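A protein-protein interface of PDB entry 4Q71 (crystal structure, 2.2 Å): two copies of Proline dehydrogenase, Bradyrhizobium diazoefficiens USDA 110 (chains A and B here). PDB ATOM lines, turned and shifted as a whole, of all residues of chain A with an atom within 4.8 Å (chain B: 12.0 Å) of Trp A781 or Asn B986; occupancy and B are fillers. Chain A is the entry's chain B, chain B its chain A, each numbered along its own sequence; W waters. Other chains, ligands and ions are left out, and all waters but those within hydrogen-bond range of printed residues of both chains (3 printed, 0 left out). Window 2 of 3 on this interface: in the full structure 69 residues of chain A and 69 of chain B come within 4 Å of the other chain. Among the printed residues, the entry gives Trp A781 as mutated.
Thr B639 touches Lys A353.
CH2 of Trp A781 touches ND2 of Asn B986 (3.9 Å).
Val A942 touches Ile B985.
CG2 of Thr B984 touches CD of Arg A944 (3.9 Å).
OD1 of Asn B643 is in hydrogen-bond range of OG1 of Thr B984 (2.7 Å).
ND2 of Asn B643 is in hydrogen-bond range of OE1 of Glu B641 (3.0 Å).
The backbone carbonyl oxygen of Gly B640 is in hydrogen-bond range of the backbone NH of Thr B987 (2.9 Å).
The side-chain amide oxygen (OD1) of Asn B986 lies within hydrogen-bond range of the backbone NH (N) of Ala B988 (3.0 Å).
NE2 of His A921 sits close to O of Arg A944.
The side-chain hydroxyl of Ser A785 lies within hydrogen-bond range of the backbone carbonyl oxygen of Trp A781 (2.5 Å).
Of the printed residues of chain A, Asn B986 touches Lys A353, Trp A781, Val A942 and Asn A943.
No residue of chain B comes within 4 Å of Ala A779.
Val A782 touches none of the printed residues of chain B.
No residue of chain B comes within 4 Å of Val A783.
Thr A784 touches none of the printed residues of chain B.
Printed residues of chain B within 4 Å of Val A942: Thr B984 (2.8 Å), Ile B985 (3.8 Å) and Asn B986 (3.0 Å).
Asn A943 touches one residue of chain B.
Of the printed residues of chain A, Thr B639 touches Lys A353 (3.3 Å).
Printed residues of chain B within 4 Å of Lys A353: Thr B639, Gly B640 and Asn B986.
Printed residues of chain A within 4 Å of Glu B641: Arg A944 (2.8 Å).
The nearest printed residue of chain A that does not touch Asn B986 is Arg A944 (4.02 Å).
Water W2 lies within hydrogen-bond range of the side-chain carboxylate of Glu B641 and the side-chain amino group of Lys A353.
Water W1 lies within hydrogen-bond range of O of Asn B986 (2.8 Å) and ND2 of Asn A943 (3.1 Å).
Water W3 bridges OE2 of Glu B641 (2.9 Å) and NH2 of Arg A944 (3.3 Å).
Of the 18 printed residues of chain B, 6 touch a printed residue of chain A.
Printed residues of chain B that touch a printed residue of chain A: Thr B639, Gly B640, Glu B641, Thr B984, Ile B985 and Asn B986.
Among the printed residues, 10 pairs touch across the chains.
No position is printed for both chains.
Of the 10 pairs that touch across the chains among the printed residues, none has its exchanged pair printed and touching as well.
OE2 of Glu B641 lies within salt-bridge range of NH2 of Arg A944, at 2.8 Å.
The backbone carbonyl oxygen of Val A942 lies within hydrogen-bond range of the backbone NH of Asn B986 (3.0 Å).
The backbone carbonyl oxygen of Gly B640 is in hydrogen-bond range of the side-chain amino group of Lys A353, at 3.0 Å.
The side-chain amide nitrogen (ND2) of Asn B986 is in hydrogen-bond range of the backbone carbonyl oxygen (O) of Asn A943 (2.9 Å).
The side-chain amide oxygen of Asn B986 lies within hydrogen-bond range of the side-chain amino group of Lys A353, 3.0 Å away.
The backbone carbonyl oxygen (O) of Thr B984 sits at hydrogen-bond distance from the backbone NH (N) of Val A942.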
ATOM      1  N   LYS A 353     -12.917 -33.995  13.991  1.00  0.00           N
ATOM      2  CA  LYS A 353     -11.775 -34.265  14.854  1.00  0.00           C
ATOM      3  C   LYS A 353     -12.206 -35.108  16.048  1.00  0.00           C
ATOM      4  O   LYS A 353     -11.502 -36.042  16.440  1.00  0.00           O
ATOM      5  CB  LYS A 353     -11.136 -32.948  15.321  1.00  0.00           C
ATOM      6  CG  LYS A 353      -9.920 -33.121  16.243  1.00  0.00           C
ATOM      7  CD  LYS A 353      -9.265 -31.782  16.532  1.00  0.00           C
ATOM      8  CE  LYS A 353      -7.974 -31.954  17.324  1.00  0.00           C
ATOM      9  NZ  LYS A 353      -7.280 -30.646  17.580  1.00  0.00           N
ATOM     10  N   MET A 767       3.281 -25.683  32.244  1.00  0.00           N
ATOM     11  CA  MET A 767       2.523 -25.134  31.131  1.00  0.00           C
ATOM     12  C   MET A 767       2.752 -23.631  31.100  1.00  0.00           C
ATOM     13  O   MET A 767       2.794 -22.980  32.141  1.00  0.00           O
ATOM     14  CB  MET A 767       1.030 -25.450  31.250  1.00  0.00           C
ATOM     15  CG  MET A 767       0.166 -24.795  30.168  1.00  0.00           C
ATOM     16  SD  MET A 767      -1.617 -25.076  30.381  1.00  0.00           S
ATOM     17  CE  MET A 767      -1.752 -26.875  30.208  1.00  0.00           C
ATOM     18  N   GLN A 777     -10.403 -21.526  27.251  1.00  0.00           N
ATOM     19  CA  GLN A 777      -9.812 -22.722  26.646  1.00  0.00           C
ATOM     20  C   GLN A 777      -8.629 -23.213  27.468  1.00  0.00           C
ATOM     21  O   GLN A 777      -8.507 -24.404  27.758  1.00  0.00           O
ATOM     22  CB  GLN A 777      -9.341 -22.395  25.221  1.00  0.00           C
ATOM     23  CG  GLN A 777      -9.932 -23.267  24.128  1.00  0.00           C
ATOM     24  CD  GLN A 777      -9.731 -22.677  22.729  1.00  0.00           C
ATOM     25  OE1 GLN A 777      -8.795 -21.903  22.490  1.00  0.00           O
ATOM     26  NE2 GLN A 777     -10.601 -23.063  21.794  1.00  0.00           N
ATOM     27  N   VAL A 778      -7.736 -22.288  27.812  1.00  0.00           N
ATOM     28  CA  VAL A 778      -6.651 -22.588  28.731  1.00  0.00           C
ATOM     29  C   VAL A 778      -7.210 -23.201  30.006  1.00  0.00           C
ATOM     30  O   VAL A 778      -6.702 -24.230  30.481  1.00  0.00           O
ATOM     31  CB  VAL A 778      -5.820 -21.325  29.079  1.00  0.00           C
ATOM     32  CG1 VAL A 778      -4.814 -21.615  30.192  1.00  0.00           C
ATOM     33  CG2 VAL A 778      -5.108 -20.822  27.843  1.00  0.00           C
ATOM     34  N   ALA A 779      -8.271 -22.596  30.543  1.00  0.00           N
ATOM     35  CA  ALA A 779      -8.879 -23.115  31.773  1.00  0.00           C
ATOM     36  C   ALA A 779      -9.359 -24.568  31.628  1.00  0.00           C
ATOM     37  O   ALA A 779      -9.122 -25.392  32.514  1.00  0.00           O
ATOM     38  CB  ALA A 779     -10.032 -22.203  32.242  1.00  0.00           C
ATOM     39  N   ASP A 780     -10.031 -24.878  30.519  1.00  0.00           N
ATOM     40  CA  ASP A 780     -10.474 -26.250  30.234  1.00  0.00           C
ATOM     41  C   ASP A 780      -9.278 -27.192  30.203  1.00  0.00           C
ATOM     42  O   ASP A 780      -9.270 -28.275  30.817  1.00  0.00           O
ATOM     43  CB  ASP A 780     -11.172 -26.318  28.865  1.00  0.00           C
ATOM     44  CG  ASP A 780     -12.639 -25.909  28.920  1.00  0.00           C
ATOM     45  OD1 ASP A 780     -13.220 -25.857  30.026  1.00  0.00           O
ATOM     46  OD2 ASP A 780     -13.213 -25.639  27.841  1.00  0.00           O
ATOM     47  N   TRP A 781      -8.244 -26.758  29.503  1.00  0.00           N
ATOM     48  CA  TRP A 781      -7.075 -27.606  29.309  1.00  0.00           C
ATOM     49  C   TRP A 781      -6.246 -27.754  30.576  1.00  0.00           C
ATOM     50  O   TRP A 781      -5.630 -28.800  30.812  1.00  0.00           O
ATOM     51  CB  TRP A 781      -6.269 -27.105  28.108  1.00  0.00           C
ATOM     52  CG  TRP A 781      -7.047 -27.343  26.824  1.00  0.00           C
ATOM     53  CD1 TRP A 781      -7.949 -28.348  26.595  1.00  0.00           C
ATOM     54  CD2 TRP A 781      -7.033 -26.542  25.631  1.00  0.00           C
ATOM     55  NE1 TRP A 781      -8.468 -28.245  25.326  1.00  0.00           N
ATOM     56  CE2 TRP A 781      -7.933 -27.138  24.716  1.00  0.00           C
ATOM     57  CE3 TRP A 781      -6.342 -25.385  25.248  1.00  0.00           C
ATOM     58  CZ2 TRP A 781      -8.159 -26.615  23.430  1.00  0.00           C
ATOM     59  CZ3 TRP A 781      -6.567 -24.862  23.971  1.00  0.00           C
ATOM     60  CH2 TRP A 781      -7.462 -25.484  23.076  1.00  0.00           C
ATOM     61  N   VAL A 782      -6.282 -26.730  31.424  1.00  0.00           N
ATOM     62  CA  VAL A 782      -5.566 -26.781  32.684  1.00  0.00           C
ATOM     63  C   VAL A 782      -6.294 -27.703  33.660  1.00  0.00           C
ATOM     64  O   VAL A 782      -5.671 -28.492  34.367  1.00  0.00           O
ATOM     65  CB  VAL A 782      -5.414 -25.364  33.310  1.00  0.00           C
ATOM     66  CG1 VAL A 782      -5.094 -25.466  34.785  1.00  0.00           C
ATOM     67  CG2 VAL A 782      -4.332 -24.583  32.586  1.00  0.00           C
ATOM     68  N   VAL A 783      -7.616 -27.591  33.698  1.00  0.00           N
ATOM     69  CA  VAL A 783      -8.423 -28.404  34.606  1.00  0.00           C
ATOM     70  C   VAL A 783      -8.272 -29.878  34.259  1.00  0.00           C
ATOM     71  O   VAL A 783      -7.986 -30.727  35.114  1.00  0.00           O
ATOM     72  CB  VAL A 783      -9.911 -27.953  34.587  1.00  0.00           C
ATOM     73  CG1 VAL A 783     -10.818 -29.036  35.133  1.00  0.00           C
ATOM     74  CG2 VAL A 783     -10.073 -26.662  35.381  1.00  0.00           C
ATOM     75  N   THR A 784      -8.444 -30.173  32.985  1.00  0.00           N
ATOM     76  CA  THR A 784      -8.201 -31.511  32.473  1.00  0.00           C
ATOM     77  C   THR A 784      -6.790 -32.018  32.784  1.00  0.00           C
ATOM     78  O   THR A 784      -6.612 -33.092  33.349  1.00  0.00           O
ATOM     79  CB  THR A 784      -8.426 -31.551  30.948  1.00  0.00           C
ATOM     80  OG1 THR A 784      -9.830 -31.457  30.675  1.00  0.00           O
ATOM     81  CG2 THR A 784      -7.877 -32.832  30.354  1.00  0.00           C
ATOM     82  N   SER A 785      -5.781 -31.238  32.416  1.00  0.00           N
ATOM     83  CA  SER A 785      -4.397 -31.703  32.543  1.00  0.00           C
ATOM     84  C   SER A 785      -3.962 -31.919  33.990  1.00  0.00           C
ATOM     85  O   SER A 785      -3.179 -32.827  34.273  1.00  0.00           O
ATOM     86  CB  SER A 785      -3.446 -30.736  31.839  1.00  0.00           C
ATOM     87  OG  SER A 785      -3.857 -30.570  30.485  1.00  0.00           O
ATOM     88  N   HIS A 921       0.593 -22.364  25.369  1.00  0.00           N
ATOM     89  CA  HIS A 921      -0.666 -21.803  24.901  1.00  0.00           C
ATOM     90  C   HIS A 921      -0.477 -20.373  24.434  1.00  0.00           C
ATOM     91  O   HIS A 921      -0.188 -19.465  25.211  1.00  0.00           O
ATOM     92  CB  HIS A 921      -1.763 -21.944  25.963  1.00  0.00           C
ATOM     93  CG  HIS A 921      -2.087 -23.370  26.275  1.00  0.00           C
ATOM     94  ND1 HIS A 921      -3.179 -24.020  25.738  1.00  0.00           N
ATOM     95  CD2 HIS A 921      -1.420 -24.295  27.009  1.00  0.00           C
ATOM     96  CE1 HIS A 921      -3.185 -25.277  26.150  1.00  0.00           C
ATOM     97  NE2 HIS A 921      -2.132 -25.468  26.925  1.00  0.00           N
ATOM     98  N   VAL A 942       0.863 -28.091  22.206  1.00  0.00           N
ATOM     99  CA  VAL A 942       0.587 -26.701  21.899  1.00  0.00           C
ATOM    100  C   VAL A 942      -0.907 -26.452  21.698  1.00  0.00           C
ATOM    101  O   VAL A 942      -1.526 -27.029  20.802  1.00  0.00           O
ATOM    102  CB  VAL A 942       1.369 -26.266  20.637  1.00  0.00           C
ATOM    103  CG1 VAL A 942       1.187 -24.779  20.370  1.00  0.00           C
ATOM    104  CG2 VAL A 942       2.842 -26.573  20.821  1.00  0.00           C
ATOM    105  N   ASN A 943      -1.477 -25.591  22.538  1.00  0.00           N
ATOM    106  CA  ASN A 943      -2.895 -25.221  22.438  1.00  0.00           C
ATOM    107  C   ASN A 943      -3.883 -26.403  22.535  1.00  0.00           C
ATOM    108  O   ASN A 943      -4.849 -26.474  21.786  1.00  0.00           O
ATOM    109  CB  ASN A 943      -3.166 -24.381  21.171  1.00  0.00           C
ATOM    110  CG  ASN A 943      -2.482 -23.007  21.214  1.00  0.00           C
ATOM    111  OD1 ASN A 943      -2.354 -22.399  22.281  1.00  0.00           O
ATOM    112  ND2 ASN A 943      -2.040 -22.518  20.046  1.00  0.00           N
ATOM    113  N   ARG A 944      -3.626 -27.314  23.468  1.00  0.00           N
ATOM    114  CA  ARG A 944      -4.547 -28.399  23.793  1.00  0.00           C
ATOM    115  C   ARG A 944      -4.140 -28.907  25.159  1.00  0.00           C
ATOM    116  O   ARG A 944      -3.232 -28.345  25.784  1.00  0.00           O
ATOM    117  CB  ARG A 944      -4.486 -29.532  22.760  1.00  0.00           C
ATOM    118  CG  ARG A 944      -3.075 -30.031  22.427  1.00  0.00           C
ATOM    119  CD  ARG A 944      -3.112 -31.469  21.938  1.00  0.00           C
ATOM    120  NE  ARG A 944      -3.263 -32.391  23.063  1.00  0.00           N
ATOM    121  CZ  ARG A 944      -3.415 -33.706  22.948  1.00  0.00           C
ATOM    122  NH1 ARG A 944      -3.527 -34.452  24.043  1.00  0.00           N
ATOM    123  NH2 ARG A 944      -3.447 -34.272  21.742  1.00  0.00           N
ATOM    124  N   ASN A 945      -4.785 -29.963  25.644  1.00  0.00           N
ATOM    125  CA  ASN A 945      -4.349 -30.499  26.934  1.00  0.00           C
ATOM    126  C   ASN A 945      -2.979 -31.202  26.842  1.00  0.00           C
ATOM    127  O   ASN A 945      -2.435 -31.374  25.739  1.00  0.00           O
ATOM    128  CB  ASN A 945      -5.442 -31.339  27.609  1.00  0.00           C
ATOM    129  CG  ASN A 945      -5.579 -32.723  27.014  1.00  0.00           C
ATOM    130  OD1 ASN A 945      -4.598 -33.320  26.570  1.00  0.00           O
ATOM    131  ND2 ASN A 945      -6.805 -33.254  27.020  1.00  0.00           N
ATOM    132  N   MET B 635       3.841 -38.006  12.350  1.00  0.00           N
ATOM    133  CA  MET B 635       3.088 -39.152  12.867  1.00  0.00           C
ATOM    134  C   MET B 635       1.651 -39.062  12.397  1.00  0.00           C
ATOM    135  O   MET B 635       1.117 -37.965  12.245  1.00  0.00           O
ATOM    136  CB  MET B 635       3.115 -39.235  14.407  1.00  0.00           C
ATOM    137  CG  MET B 635       4.477 -39.054  15.054  1.00  0.00           C
ATOM    138  SD  MET B 635       5.703 -40.282  14.561  1.00  0.00           S
ATOM    139  CE  MET B 635       4.912 -41.787  15.128  1.00  0.00           C
ATOM    140  N   GLY B 637      -2.403 -39.199  12.690  1.00  0.00           N
ATOM    141  CA  GLY B 637      -3.220 -38.699  13.761  1.00  0.00           C
ATOM    142  C   GLY B 637      -4.506 -38.102  13.271  1.00  0.00           C
ATOM    143  O   GLY B 637      -4.865 -38.229  12.104  1.00  0.00           O
ATOM    144  N   PRO B 638      -5.216 -37.435  14.177  1.00  0.00           N
ATOM    145  CA  PRO B 638      -6.517 -36.891  13.819  1.00  0.00           C
ATOM    146  C   PRO B 638      -6.312 -35.650  12.975  1.00  0.00           C
ATOM    147  O   PRO B 638      -5.213 -35.088  12.993  1.00  0.00           O
ATOM    148  CB  PRO B 638      -7.134 -36.545  15.182  1.00  0.00           C
ATOM    149  CG  PRO B 638      -5.944 -36.272  16.072  1.00  0.00           C
ATOM    150  CD  PRO B 638      -4.862 -37.197  15.589  1.00  0.00           C
ATOM    151  N   THR B 639      -7.326 -35.288  12.196  1.00  0.00           N
ATOM    152  CA  THR B 639      -7.379 -34.009  11.503  1.00  0.00           C
ATOM    153  C   THR B 639      -7.365 -32.862  12.543  1.00  0.00           C
ATOM    154  O   THR B 639      -7.774 -33.055  13.700  1.00  0.00           O
ATOM    155  CB  THR B 639      -8.678 -33.918  10.655  1.00  0.00           C
ATOM    156  OG1 THR B 639      -8.689 -32.702   9.901  1.00  0.00           O
ATOM    157  CG2 THR B 639      -9.912 -33.936  11.554  1.00  0.00           C
ATOM    158  N   GLY B 640      -6.901 -31.679  12.140  1.00  0.00           N
ATOM    159  CA  GLY B 640      -6.825 -30.539  13.042  1.00  0.00           C
ATOM    160  C   GLY B 640      -5.730 -30.644  14.101  1.00  0.00           C
ATOM    161  O   GLY B 640      -5.777 -29.961  15.126  1.00  0.00           O
ATOM    162  N   GLU B 641      -4.734 -31.489  13.855  1.00  0.00           N
ATOM    163  CA  GLU B 641      -3.623 -31.644  14.787  1.00  0.00           C
ATOM    164  C   GLU B 641      -2.403 -32.151  14.046  1.00  0.00           C
ATOM    165  O   GLU B 641      -2.514 -33.034  13.201  1.00  0.00           O
ATOM    166  CB  GLU B 641      -4.001 -32.627  15.909  1.00  0.00           C
ATOM    167  CG  GLU B 641      -3.020 -32.696  17.067  1.00  0.00           C
ATOM    168  CD  GLU B 641      -3.384 -33.775  18.087  1.00  0.00           C
ATOM    169  OE1 GLU B 641      -3.102 -34.974  17.817  1.00  0.00           O
ATOM    170  OE2 GLU B 641      -3.960 -33.423  19.143  1.00  0.00           O
ATOM    171  N   SER B 642      -1.232 -31.615  14.378  1.00  0.00           N
ATOM    172  CA  SER B 642      -0.001 -32.124  13.800  1.00  0.00           C
ATOM    173  C   SER B 642       0.842 -32.765  14.893  1.00  0.00           C
ATOM    174  O   SER B 642       0.867 -32.305  16.046  1.00  0.00           O
ATOM    175  CB  SER B 642       0.793 -31.019  13.100  1.00  0.00           C
ATOM    176  OG  SER B 642       1.346 -30.108  14.038  1.00  0.00           O
ATOM    177  N   ASN B 643       1.513 -33.838  14.517  1.00  0.00           N
ATOM    178  CA  ASN B 643       2.379 -34.572  15.419  1.00  0.00           C
ATOM    179  C   ASN B 643       3.675 -34.850  14.701  1.00  0.00           C
ATOM    180  O   ASN B 643       3.676 -35.496  13.647  1.00  0.00           O
ATOM    181  CB  ASN B 643       1.723 -35.869  15.893  1.00  0.00           C
ATOM    182  CG  ASN B 643       0.511 -35.617  16.768  1.00  0.00           C
ATOM    183  OD1 ASN B 643       0.640 -35.440  17.982  1.00  0.00           O
ATOM    184  ND2 ASN B 643      -0.673 -35.585  16.157  1.00  0.00           N
ATOM    185  N   ALA B 644       4.764 -34.315  15.249  1.00  0.00           N
ATOM    186  CA  ALA B 644       6.087 -34.440  14.646  1.00  0.00           C
ATOM    187  C   ALA B 644       7.078 -34.985  15.655  1.00  0.00           C
ATOM    188  O   ALA B 644       7.135 -34.524  16.800  1.00  0.00           O
ATOM    189  CB  ALA B 644       6.564 -33.098  14.114  1.00  0.00           C
ATOM    190  N   THR B 982       8.609 -35.192  20.853  1.00  0.00           N
ATOM    191  CA  THR B 982       7.353 -35.109  20.123  1.00  0.00           C
ATOM    192  C   THR B 982       6.732 -33.741  20.302  1.00  0.00           C
ATOM    193  O   THR B 982       6.555 -33.270  21.432  1.00  0.00           O
ATOM    194  CB  THR B 982       6.356 -36.162  20.626  1.00  0.00           C
ATOM    195  OG1 THR B 982       6.971 -37.457  20.577  1.00  0.00           O
ATOM    196  CG2 THR B 982       5.088 -36.156  19.779  1.00  0.00           C
ATOM    197  N   VAL B 983       6.392 -33.103  19.187  1.00  0.00           N
ATOM    198  CA  VAL B 983       5.675 -31.838  19.224  1.00  0.00           C
ATOM    199  C   VAL B 983       4.280 -32.018  18.652  1.00  0.00           C
ATOM    200  O   VAL B 983       4.107 -32.426  17.494  1.00  0.00           O
ATOM    201  CB  VAL B 983       6.390 -30.730  18.440  1.00  0.00           C
ATOM    202  CG1 VAL B 983       5.471 -29.495  18.335  1.00  0.00           C
ATOM    203  CG2 VAL B 983       7.706 -30.381  19.108  1.00  0.00           C
ATOM    204  N   THR B 984       3.287 -31.743  19.482  1.00  0.00           N
ATOM    205  CA  THR B 984       1.902 -31.907  19.105  1.00  0.00           C
ATOM    206  C   THR B 984       1.231 -30.538  19.100  1.00  0.00           C
ATOM    207  O   THR B 984       1.171 -29.866  20.126  1.00  0.00           O
ATOM    208  CB  THR B 984       1.162 -32.841  20.089  1.00  0.00           C
ATOM    209  OG1 THR B 984       1.785 -34.127  20.098  1.00  0.00           O
ATOM    210  CG2 THR B 984      -0.318 -32.981  19.712  1.00  0.00           C
ATOM    211  N   ILE B 985       0.737 -30.122  17.939  1.00  0.00           N
ATOM    212  CA  ILE B 985       0.102 -28.824  17.815  1.00  0.00           C
ATOM    213  C   ILE B 985      -1.354 -28.946  17.375  1.00  0.00           C
ATOM    214  O   ILE B 985      -1.639 -29.501  16.320  1.00  0.00           O
ATOM    215  CB  ILE B 985       0.838 -27.937  16.794  1.00  0.00           C
ATOM    216  CG1 ILE B 985       2.318 -27.807  17.168  1.00  0.00           C
ATOM    217  CG2 ILE B 985       0.145 -26.567  16.690  1.00  0.00           C
ATOM    218  CD1 ILE B 985       3.162 -27.095  16.127  1.00  0.00           C
ATOM    219  N   ASN B 986      -2.261 -28.416  18.194  1.00  0.00           N
ATOM    220  CA  ASN B 986      -3.662 -28.300  17.818  1.00  0.00           C
ATOM    221  C   ASN B 986      -3.804 -27.238  16.726  1.00  0.00           C
ATOM    222  O   ASN B 986      -3.736 -26.039  16.990  1.00  0.00           O
ATOM    223  CB  ASN B 986      -4.504 -27.972  19.059  1.00  0.00           C
ATOM    224  CG  ASN B 986      -5.978 -27.692  18.744  1.00  0.00           C
ATOM    225  OD1 ASN B 986      -6.414 -27.728  17.593  1.00  0.00           O
ATOM    226  ND2 ASN B 986      -6.749 -27.413  19.790  1.00  0.00           N
ATOM    227  N   THR B 987      -3.997 -27.685  15.494  1.00  0.00           N
ATOM    228  CA  THR B 987      -4.003 -26.760  14.371  1.00  0.00           C
ATOM    229  C   THR B 987      -5.400 -26.305  13.995  1.00  0.00           C
ATOM    230  O   THR B 987      -5.562 -25.555  13.029  1.00  0.00           O
ATOM    231  CB  THR B 987      -3.309 -27.364  13.132  1.00  0.00           C
ATOM    232  OG1 THR B 987      -4.003 -28.546  12.700  1.00  0.00           O
ATOM    233  CG2 THR B 987      -1.857 -27.712  13.455  1.00  0.00           C
ATOM    234  N   ALA B 988      -6.399 -26.728  14.771  1.00  0.00           N
ATOM    235  CA  ALA B 988      -7.802 -26.484  14.412  1.00  0.00           C
ATOM    236  C   ALA B 988      -8.178 -25.011  14.277  1.00  0.00           C
ATOM    237  O   ALA B 988      -9.080 -24.668  13.500  1.00  0.00           O
ATOM    238  CB  ALA B 988      -8.743 -27.182  15.369  1.00  0.00           C
ATOM    239  N   ALA B 989      -7.502 -24.148  15.034  1.00  0.00           N
ATOM    240  CA  ALA B 989      -7.740 -22.705  14.953  1.00  0.00           C
ATOM    241  C   ALA B 989      -7.473 -22.175  13.536  1.00  0.00           C
ATOM    242  O   ALA B 989      -8.130 -21.232  13.082  1.00  0.00           O
ATOM    243  CB  ALA B 989      -6.888 -21.967  15.979  1.00  0.00           C
ATOM    244  N   ALA B 990      -6.508 -22.789  12.850  1.00  0.00           N
ATOM    245  CA  ALA B 990      -6.249 -22.516  11.439  1.00  0.00           C
ATOM    246  C   ALA B 990      -7.329 -23.147  10.569  1.00  0.00           C
ATOM    247  O   ALA B 990      -7.637 -22.650   9.486  1.00  0.00           O
ATOM    248  CB  ALA B 990      -4.877 -23.044  11.035  1.00  0.00           C
HETATM  249  O   HOH W   1      -1.871 -23.946  17.289  1.00  0.00           O
HETATM  250  O   HOH W   2      -5.236 -31.089  19.312  1.00  0.00           O
HETATM  251  O   HOH W   3      -6.365 -34.578  20.172  1.00  0.00           O
